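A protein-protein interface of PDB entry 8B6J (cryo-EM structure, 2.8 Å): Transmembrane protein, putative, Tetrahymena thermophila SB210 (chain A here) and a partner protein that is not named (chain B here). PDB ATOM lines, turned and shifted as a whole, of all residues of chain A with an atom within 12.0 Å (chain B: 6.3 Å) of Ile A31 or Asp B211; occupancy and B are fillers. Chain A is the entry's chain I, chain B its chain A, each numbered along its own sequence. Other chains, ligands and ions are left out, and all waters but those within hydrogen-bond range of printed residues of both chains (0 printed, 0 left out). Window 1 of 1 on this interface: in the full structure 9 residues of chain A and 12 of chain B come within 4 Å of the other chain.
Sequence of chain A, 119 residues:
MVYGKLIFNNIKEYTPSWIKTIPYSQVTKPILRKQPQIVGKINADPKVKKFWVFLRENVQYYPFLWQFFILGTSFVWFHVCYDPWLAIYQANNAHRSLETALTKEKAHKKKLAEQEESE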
ATOM      1  N   TYR A  24     -22.787 -32.961  -4.913  1.00  0.00           N
ATOM      2  CA  TYR A  24     -22.861 -32.505  -6.296  1.00  0.00           C
ATOM      3  C   TYR A  24     -23.481 -31.122  -6.423  1.00  0.00           C
ATOM      4  O   TYR A  24     -23.295 -30.467  -7.452  1.00  0.00           O
ATOM      5  CB  TYR A  24     -23.654 -33.504  -7.137  1.00  0.00           C
ATOM      6  CG  TYR A  24     -23.857 -33.069  -8.570  1.00  0.00           C
ATOM      7  CD1 TYR A  24     -22.835 -33.184  -9.502  1.00  0.00           C
ATOM      8  CD2 TYR A  24     -25.070 -32.545  -8.991  1.00  0.00           C
ATOM      9  CE1 TYR A  24     -23.015 -32.788 -10.811  1.00  0.00           C
ATOM     10  CE2 TYR A  24     -25.259 -32.147 -10.299  1.00  0.00           C
ATOM     11  CZ  TYR A  24     -24.229 -32.271 -11.204  1.00  0.00           C
ATOM     12  OH  TYR A  24     -24.414 -31.875 -12.508  1.00  0.00           O
ATOM     13  N   VAL A  27     -20.574 -28.416  -6.884  1.00  0.00           N
ATOM     14  CA  VAL A  27     -19.610 -28.498  -7.975  1.00  0.00           C
ATOM     15  C   VAL A  27     -20.042 -27.547  -9.082  1.00  0.00           C
ATOM     16  O   VAL A  27     -21.216 -27.524  -9.472  1.00  0.00           O
ATOM     17  CB  VAL A  27     -19.483 -29.938  -8.499  1.00  0.00           C
ATOM     18  CG1 VAL A  27     -19.257 -30.907  -7.349  1.00  0.00           C
ATOM     19  CG2 VAL A  27     -20.710 -30.327  -9.299  1.00  0.00           C
ATOM     20  N   THR A  28     -19.099 -26.754  -9.582  1.00  0.00           N
ATOM     21  CA  THR A  28     -19.407 -25.792 -10.631  1.00  0.00           C
ATOM     22  C   THR A  28     -19.681 -26.515 -11.943  1.00  0.00           C
ATOM     23  O   THR A  28     -18.896 -27.366 -12.372  1.00  0.00           O
ATOM     24  CB  THR A  28     -18.252 -24.808 -10.805  1.00  0.00           C
ATOM     25  OG1 THR A  28     -17.066 -25.518 -11.179  1.00  0.00           O
ATOM     26  CG2 THR A  28     -17.996 -24.050  -9.512  1.00  0.00           C
ATOM     27  N   LYS A  29     -20.796 -26.172 -12.581  1.00  0.00           N
ATOM     28  CA  LYS A  29     -21.183 -26.829 -13.818  1.00  0.00           C
ATOM     29  C   LYS A  29     -20.430 -26.224 -15.001  1.00  0.00           C
ATOM     30  O   LYS A  29     -20.021 -25.061 -14.957  1.00  0.00           O
ATOM     31  CB  LYS A  29     -22.684 -26.699 -14.051  1.00  0.00           C
ATOM     32  CG  LYS A  29     -23.538 -26.733 -12.793  1.00  0.00           C
ATOM     33  CD  LYS A  29     -23.282 -27.967 -11.947  1.00  0.00           C
ATOM     34  CE  LYS A  29     -24.215 -27.996 -10.746  1.00  0.00           C
ATOM     35  NZ  LYS A  29     -23.894 -29.091  -9.798  1.00  0.00           N
ATOM     36  N   PRO A  30     -20.235 -26.991 -16.071  1.00  0.00           N
ATOM     37  CA  PRO A  30     -19.561 -26.446 -17.251  1.00  0.00           C
ATOM     38  C   PRO A  30     -20.453 -25.482 -18.018  1.00  0.00           C
ATOM     39  O   PRO A  30     -21.683 -25.538 -17.954  1.00  0.00           O
ATOM     40  CB  PRO A  30     -19.246 -27.692 -18.083  1.00  0.00           C
ATOM     41  CG  PRO A  30     -20.319 -28.651 -17.716  1.00  0.00           C
ATOM     42  CD  PRO A  30     -20.636 -28.395 -16.267  1.00  0.00           C
ATOM     43  N   ILE A  31     -19.806 -24.585 -18.753  1.00  0.00           N
ATOM     44  CA  ILE A  31     -20.497 -23.674 -19.658  1.00  0.00           C
ATOM     45  C   ILE A  31     -20.596 -24.359 -21.015  1.00  0.00           C
ATOM     46  O   ILE A  31     -19.576 -24.684 -21.632  1.00  0.00           O
ATOM     47  CB  ILE A  31     -19.760 -22.331 -19.770  1.00  0.00           C
ATOM     48  CG1 ILE A  31     -19.577 -21.695 -18.388  1.00  0.00           C
ATOM     49  CG2 ILE A  31     -20.514 -21.387 -20.693  1.00  0.00           C
ATOM     50  CD1 ILE A  31     -20.874 -21.389 -17.664  1.00  0.00           C
ATOM     51  N   LEU A  32     -21.824 -24.573 -21.485  1.00  0.00           N
ATOM     52  CA  LEU A  32     -22.086 -25.345 -22.694  1.00  0.00           C
ATOM     53  C   LEU A  32     -22.540 -24.450 -23.842  1.00  0.00           C
ATOM     54  O   LEU A  32     -23.420 -24.813 -24.625  1.00  0.00           O
ATOM     55  CB  LEU A  32     -23.122 -26.433 -22.425  1.00  0.00           C
ATOM     56  CG  LEU A  32     -22.790 -27.428 -21.311  1.00  0.00           C
ATOM     57  CD1 LEU A  32     -23.794 -28.565 -21.306  1.00  0.00           C
ATOM     58  CD2 LEU A  32     -21.374 -27.967 -21.447  1.00  0.00           C
ATOM     59  N   ARG A  33     -21.940 -23.268 -23.948  1.00  0.00           N
ATOM     60  CA  ARG A  33     -22.168 -22.364 -25.064  1.00  0.00           C
ATOM     61  C   ARG A  33     -20.829 -21.827 -25.543  1.00  0.00           C
ATOM     62  O   ARG A  33     -19.868 -21.740 -24.773  1.00  0.00           O
ATOM     63  CB  ARG A  33     -23.091 -21.202 -24.672  1.00  0.00           C
ATOM     64  CG  ARG A  33     -22.465 -20.212 -23.702  1.00  0.00           C
ATOM     65  CD  ARG A  33     -23.477 -19.191 -23.218  1.00  0.00           C
ATOM     66  NE  ARG A  33     -24.498 -19.797 -22.371  1.00  0.00           N
ATOM     67  CZ  ARG A  33     -24.393 -19.949 -21.057  1.00  0.00           C
ATOM     68  NH1 ARG A  33     -23.319 -19.547 -20.396  1.00  0.00           N
ATOM     69  NH2 ARG A  33     -25.392 -20.519 -20.389  1.00  0.00           N
ATOM     70  N   LYS A  34     -20.768 -21.471 -26.822  1.00  0.00           N
ATOM     71  CA  LYS A  34     -19.551 -20.912 -27.389  1.00  0.00           C
ATOM     72  C   LYS A  34     -19.383 -19.466 -26.941  1.00  0.00           C
ATOM     73  O   LYS A  34     -20.333 -18.679 -26.986  1.00  0.00           O
ATOM     74  CB  LYS A  34     -19.581 -20.995 -28.914  1.00  0.00           C
ATOM     75  CG  LYS A  34     -18.324 -20.455 -29.569  1.00  0.00           C
ATOM     76  CD  LYS A  34     -18.033 -21.148 -30.886  1.00  0.00           C
ATOM     77  CE  LYS A  34     -16.640 -20.812 -31.385  1.00  0.00           C
ATOM     78  NZ  LYS A  34     -16.232 -21.697 -32.507  1.00  0.00           N
ATOM     79  N   GLN A  35     -18.167 -19.120 -26.505  1.00  0.00           N
ATOM     80  CA  GLN A  35     -17.871 -17.780 -26.028  1.00  0.00           C
ATOM     81  C   GLN A  35     -17.108 -16.991 -27.087  1.00  0.00           C
ATOM     82  O   GLN A  35     -16.437 -17.576 -27.941  1.00  0.00           O
ATOM     83  CB  GLN A  35     -17.042 -17.840 -24.743  1.00  0.00           C
ATOM     84  CG  GLN A  35     -17.750 -18.523 -23.585  1.00  0.00           C
ATOM     85  CD  GLN A  35     -16.906 -18.572 -22.328  1.00  0.00           C
ATOM     86  OE1 GLN A  35     -16.793 -19.615 -21.685  1.00  0.00           O
ATOM     87  NE2 GLN A  35     -16.312 -17.440 -21.968  1.00  0.00           N
ATOM     88  N   PRO A  36     -17.192 -15.661 -27.061  1.00  0.00           N
ATOM     89  CA  PRO A  36     -16.512 -14.867 -28.091  1.00  0.00           C
ATOM     90  C   PRO A  36     -15.011 -15.116 -28.094  1.00  0.00           C
ATOM     91  O   PRO A  36     -14.383 -15.270 -27.046  1.00  0.00           O
ATOM     92  CB  PRO A  36     -16.847 -13.420 -27.705  1.00  0.00           C
ATOM     93  CG  PRO A  36     -17.249 -13.479 -26.273  1.00  0.00           C
ATOM     94  CD  PRO A  36     -17.901 -14.810 -26.091  1.00  0.00           C
ATOM     95  N   GLN A  37     -14.443 -15.151 -29.295  1.00  0.00           N
ATOM     96  CA  GLN A  37     -13.016 -15.397 -29.449  1.00  0.00           C
ATOM     97  C   GLN A  37     -12.207 -14.199 -28.968  1.00  0.00           C
ATOM     98  O   GLN A  37     -12.618 -13.046 -29.122  1.00  0.00           O
ATOM     99  CB  GLN A  37     -12.691 -15.692 -30.913  1.00  0.00           C
ATOM    100  CG  GLN A  37     -11.217 -15.937 -31.197  1.00  0.00           C
ATOM    101  CD  GLN A  37     -10.936 -16.142 -32.671  1.00  0.00           C
ATOM    102  OE1 GLN A  37     -11.846 -16.115 -33.498  1.00  0.00           O
ATOM    103  NE2 GLN A  37      -9.668 -16.345 -33.010  1.00  0.00           N
ATOM    104  N   ILE A  38     -11.047 -14.480 -28.378  1.00  0.00           N
ATOM    105  CA  ILE A  38     -10.094 -13.439 -27.992  1.00  0.00           C
ATOM    106  C   ILE A  38      -9.130 -13.299 -29.166  1.00  0.00           C
ATOM    107  O   ILE A  38      -8.127 -14.007 -29.266  1.00  0.00           O
ATOM    108  CB  ILE A  38      -9.377 -13.766 -26.685  1.00  0.00           C
ATOM    109  CG1 ILE A  38     -10.337 -13.668 -25.496  1.00  0.00           C
ATOM    110  CG2 ILE A  38      -8.197 -12.829 -26.480  1.00  0.00           C
ATOM    111  CD1 ILE A  38     -11.340 -14.795 -25.414  1.00  0.00           C
ATOM    112  N   PHE B 206     -16.762 -36.827 -24.487  1.00  0.00           N
ATOM    113  CA  PHE B 206     -16.642 -35.776 -23.481  1.00  0.00           C
ATOM    114  C   PHE B 206     -15.479 -34.843 -23.797  1.00  0.00           C
ATOM    115  O   PHE B 206     -15.640 -33.618 -23.824  1.00  0.00           O
ATOM    116  CB  PHE B 206     -16.468 -36.404 -22.098  1.00  0.00           C
ATOM    117  CG  PHE B 206     -16.318 -35.404 -20.986  1.00  0.00           C
ATOM    118  CD1 PHE B 206     -15.090 -34.828 -20.713  1.00  0.00           C
ATOM    119  CD2 PHE B 206     -17.403 -35.050 -20.206  1.00  0.00           C
ATOM    120  CE1 PHE B 206     -14.951 -33.913 -19.692  1.00  0.00           C
ATOM    121  CE2 PHE B 206     -17.268 -34.137 -19.183  1.00  0.00           C
ATOM    122  CZ  PHE B 206     -16.041 -33.567 -18.926  1.00  0.00           C
ATOM    123  N   ALA B 208     -13.788 -34.460 -26.586  1.00  0.00           N
ATOM    124  CA  ALA B 208     -13.798 -33.859 -27.914  1.00  0.00           C
ATOM    125  C   ALA B 208     -14.676 -32.617 -27.969  1.00  0.00           C
ATOM    126  O   ALA B 208     -14.364 -31.674 -28.703  1.00  0.00           O
ATOM    127  CB  ALA B 208     -14.266 -34.882 -28.947  1.00  0.00           C
ATOM    128  N   TYR B 209     -15.776 -32.597 -27.215  1.00  0.00           N
ATOM    129  CA  TYR B 209     -16.716 -31.476 -27.202  1.00  0.00           C
ATOM    130  C   TYR B 209     -16.877 -31.021 -25.754  1.00  0.00           C
ATOM    131  O   TYR B 209     -17.786 -31.470 -25.050  1.00  0.00           O
ATOM    132  CB  TYR B 209     -18.051 -31.877 -27.821  1.00  0.00           C
ATOM    133  CG  TYR B 209     -17.913 -32.618 -29.131  1.00  0.00           C
ATOM    134  CD1 TYR B 209     -17.664 -31.939 -30.313  1.00  0.00           C
ATOM    135  CD2 TYR B 209     -18.031 -33.998 -29.183  1.00  0.00           C
ATOM    136  CE1 TYR B 209     -17.535 -32.612 -31.508  1.00  0.00           C
ATOM    137  CE2 TYR B 209     -17.906 -34.680 -30.375  1.00  0.00           C
ATOM    138  CZ  TYR B 209     -17.658 -33.981 -31.535  1.00  0.00           C
ATOM    139  OH  TYR B 209     -17.532 -34.656 -32.724  1.00  0.00           O
ATOM    140  N   ARG B 210     -15.995 -30.128 -25.313  1.00  0.00           N
ATOM    141  CA  ARG B 210     -16.030 -29.620 -23.950  1.00  0.00           C
ATOM    142  C   ARG B 210     -16.898 -28.379 -23.793  1.00  0.00           C
ATOM    143  O   ARG B 210     -17.122 -27.942 -22.660  1.00  0.00           O
ATOM    144  CB  ARG B 210     -14.611 -29.298 -23.473  1.00  0.00           C
ATOM    145  CG  ARG B 210     -13.703 -30.508 -23.368  1.00  0.00           C
ATOM    146  CD  ARG B 210     -12.339 -30.117 -22.831  1.00  0.00           C
ATOM    147  NE  ARG B 210     -11.462 -31.268 -22.662  1.00  0.00           N
ATOM    148  CZ  ARG B 210     -11.464 -32.064 -21.602  1.00  0.00           C
ATOM    149  NH1 ARG B 210     -12.304 -31.875 -20.597  1.00  0.00           N
ATOM    150  NH2 ARG B 210     -10.605 -33.077 -21.551  1.00  0.00           N
ATOM    151  N   ASP B 211     -17.390 -27.805 -24.889  1.00  0.00           N
ATOM    152  CA  ASP B 211     -18.209 -26.600 -24.851  1.00  0.00           C
ATOM    153  C   ASP B 211     -19.592 -26.854 -25.439  1.00  0.00           C
ATOM    154  O   ASP B 211     -20.244 -25.934 -25.936  1.00  0.00           O
ATOM    155  CB  ASP B 211     -17.515 -25.458 -25.591  1.00  0.00           C
ATOM    156  CG  ASP B 211     -16.109 -25.205 -25.085  1.00  0.00           C
ATOM    157  OD1 ASP B 211     -15.851 -25.458 -23.889  1.00  0.00           O
ATOM    158  OD2 ASP B 211     -15.262 -24.754 -25.882  1.00  0.00           O
ATOM    159  N   HIS B 212     -20.050 -28.101 -25.389  1.00  0.00           N
ATOM    160  CA  HIS B 212     -21.338 -28.477 -25.947  1.00  0.00           C
ATOM    161  C   HIS B 212     -21.892 -29.635 -25.134  1.00  0.00           C
ATOM    162  O   HIS B 212     -21.137 -30.445 -24.591  1.00  0.00           O
ATOM    163  CB  HIS B 212     -21.207 -28.866 -27.426  1.00  0.00           C
ATOM    164  CG  HIS B 212     -22.476 -28.731 -28.206  1.00  0.00           C
ATOM    165  ND1 HIS B 212     -23.429 -29.723 -28.260  1.00  0.00           N
ATOM    166  CD2 HIS B 212     -22.944 -27.721 -28.978  1.00  0.00           C
ATOM    167  CE1 HIS B 212     -24.432 -29.329 -29.023  1.00  0.00           C
ATOM    168  NE2 HIS B 212     -24.162 -28.118 -29.472  1.00  0.00           N
ATOM    169  N   TYR B 213     -23.220 -29.707 -25.047  1.00  0.00           N
ATOM    170  CA  TYR B 213     -23.844 -30.832 -24.363  1.00  0.00           C
ATOM    171  C   TYR B 213     -23.633 -32.141 -25.106  1.00  0.00           C
ATOM    172  O   TYR B 213     -23.893 -33.209 -24.541  1.00  0.00           O
ATOM    173  CB  TYR B 213     -25.340 -30.581 -24.177  1.00  0.00           C
ATOM    174  CG  TYR B 213     -25.997 -31.560 -23.232  1.00  0.00           C
ATOM    175  CD1 TYR B 213     -26.013 -31.327 -21.866  1.00  0.00           C
ATOM    176  CD2 TYR B 213     -26.590 -32.719 -23.704  1.00  0.00           C
ATOM    177  CE1 TYR B 213     -26.607 -32.220 -20.997  1.00  0.00           C
ATOM    178  CE2 TYR B 213     -27.183 -33.617 -22.842  1.00  0.00           C
ATOM    179  CZ  TYR B 213     -27.191 -33.363 -21.492  1.00  0.00           C
ATOM    180  OH  TYR B 213     -27.784 -34.257 -20.634  1.00  0.00           O
ATOM    181  N   GLU B 283     -26.615 -25.824 -31.829  1.00  0.00           N
ATOM    182  CA  GLU B 283     -25.446 -25.264 -32.491  1.00  0.00           C
ATOM    183  C   GLU B 283     -24.419 -26.359 -32.778  1.00  0.00           C
ATOM    184  O   GLU B 283     -24.486 -27.470 -32.247  1.00  0.00           O
ATOM    185  CB  GLU B 283     -24.825 -24.149 -31.644  1.00  0.00           C
ATOM    186  CG  GLU B 283     -24.228 -24.588 -30.308  1.00  0.00           C
ATOM    187  CD  GLU B 283     -25.269 -24.766 -29.222  1.00  0.00           C
ATOM    188  OE1 GLU B 283     -26.475 -24.764 -29.547  1.00  0.00           O
ATOM    189  OE2 GLU B 283     -24.882 -24.909 -28.043  1.00  0.00           O
ATOM    190  N   TYR B 286     -18.338 -27.713 -31.977  1.00  0.00           N
ATOM    191  CA  TYR B 286     -16.974 -27.527 -32.455  1.00  0.00           C
ATOM    192  C   TYR B 286     -16.015 -28.460 -31.725  1.00  0.00           C
ATOM    193  O   TYR B 286     -16.084 -28.624 -30.505  1.00  0.00           O
ATOM    194  CB  TYR B 286     -16.541 -26.074 -32.269  1.00  0.00           C
ATOM    195  CG  TYR B 286     -17.265 -25.110 -33.179  1.00  0.00           C
ATOM    196  CD1 TYR B 286     -16.861 -24.932 -34.493  1.00  0.00           C
ATOM    197  CD2 TYR B 286     -18.353 -24.381 -32.725  1.00  0.00           C
ATOM    198  CE1 TYR B 286     -17.519 -24.057 -35.329  1.00  0.00           C
ATOM    199  CE2 TYR B 286     -19.017 -23.502 -33.553  1.00  0.00           C
ATOM    200  CZ  TYR B 286     -18.595 -23.343 -34.854  1.00  0.00           C
ATOM    201  OH  TYR B 286     -19.255 -22.467 -35.685  1.00  0.00           O
ATOM    202  N   THR B 288     -12.968 -29.936 -29.835  1.00  0.00           N
ATOM    203  CA  THR B 288     -12.077 -29.377 -28.817  1.00  0.00           C
ATOM    204  C   THR B 288     -10.950 -30.360 -28.532  1.00  0.00           C
ATOM    205  O   THR B 288     -11.124 -31.287 -27.720  1.00  0.00           O
ATOM    206  CB  THR B 288     -12.848 -29.066 -27.536  1.00  0.00           C
ATOM    207  OG1 THR B 288     -13.791 -28.017 -27.783  1.00  0.00           O
ATOM    208  CG2 THR B 288     -11.901 -28.641 -26.427  1.00  0.00           C
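A ring nitrogen (NE2) of His B212 lies within hydrogen-bond range of the backbone carbonyl oxygen (O) of Glu B283 (2.9 Å).
Among the printed residues, merely in contact across the chains: Ile A31 with Asp B211, Leu A32 with Asp B211, Leu A32 with Tyr B213, Leu A32 with Glu B283, Arg A33 with Asp B211 and Lys A34 with Tyr B286.
Tyr A24 touches none of the printed residues of chain B.
Thr A28 touches none of the printed residues of chain B.
Printed residues of chain B within 4 Å of Ile A31: Asp B211 (3.99 Å).
Of the printed residues of chain B, Leu A32 touches Asp B211 (3.4 Å), Tyr B213 (3.6 Å) and Glu B283 (3.7 Å).
Of the printed residues of chain B, Arg A33 touches Asp B211.
Of the printed residues of chain A, Asp B211 touches Ile A31 (3.99 Å), Leu A32 (3.4 Å) and Arg A33 (3.7 Å).
Printed residues of chain A within 4 Å of Glu B283: Leu A32 (3.7 Å).
Printed residues of chain A within 4 Å of Tyr B286: Lys A34.
No residue of chain A comes within 4 Å of Thr B288.
Printed residues of chain B that touch a printed residue of chain A: Asp B211, Tyr B213, Glu B283 and Tyr B286.
Hydrophobic or aromatic side chains of chain B that line the printed part of chain A: Tyr B213 and Tyr B286.
Along chain B the printed residues that touch a printed residue of chain A span positions 211 to 286.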
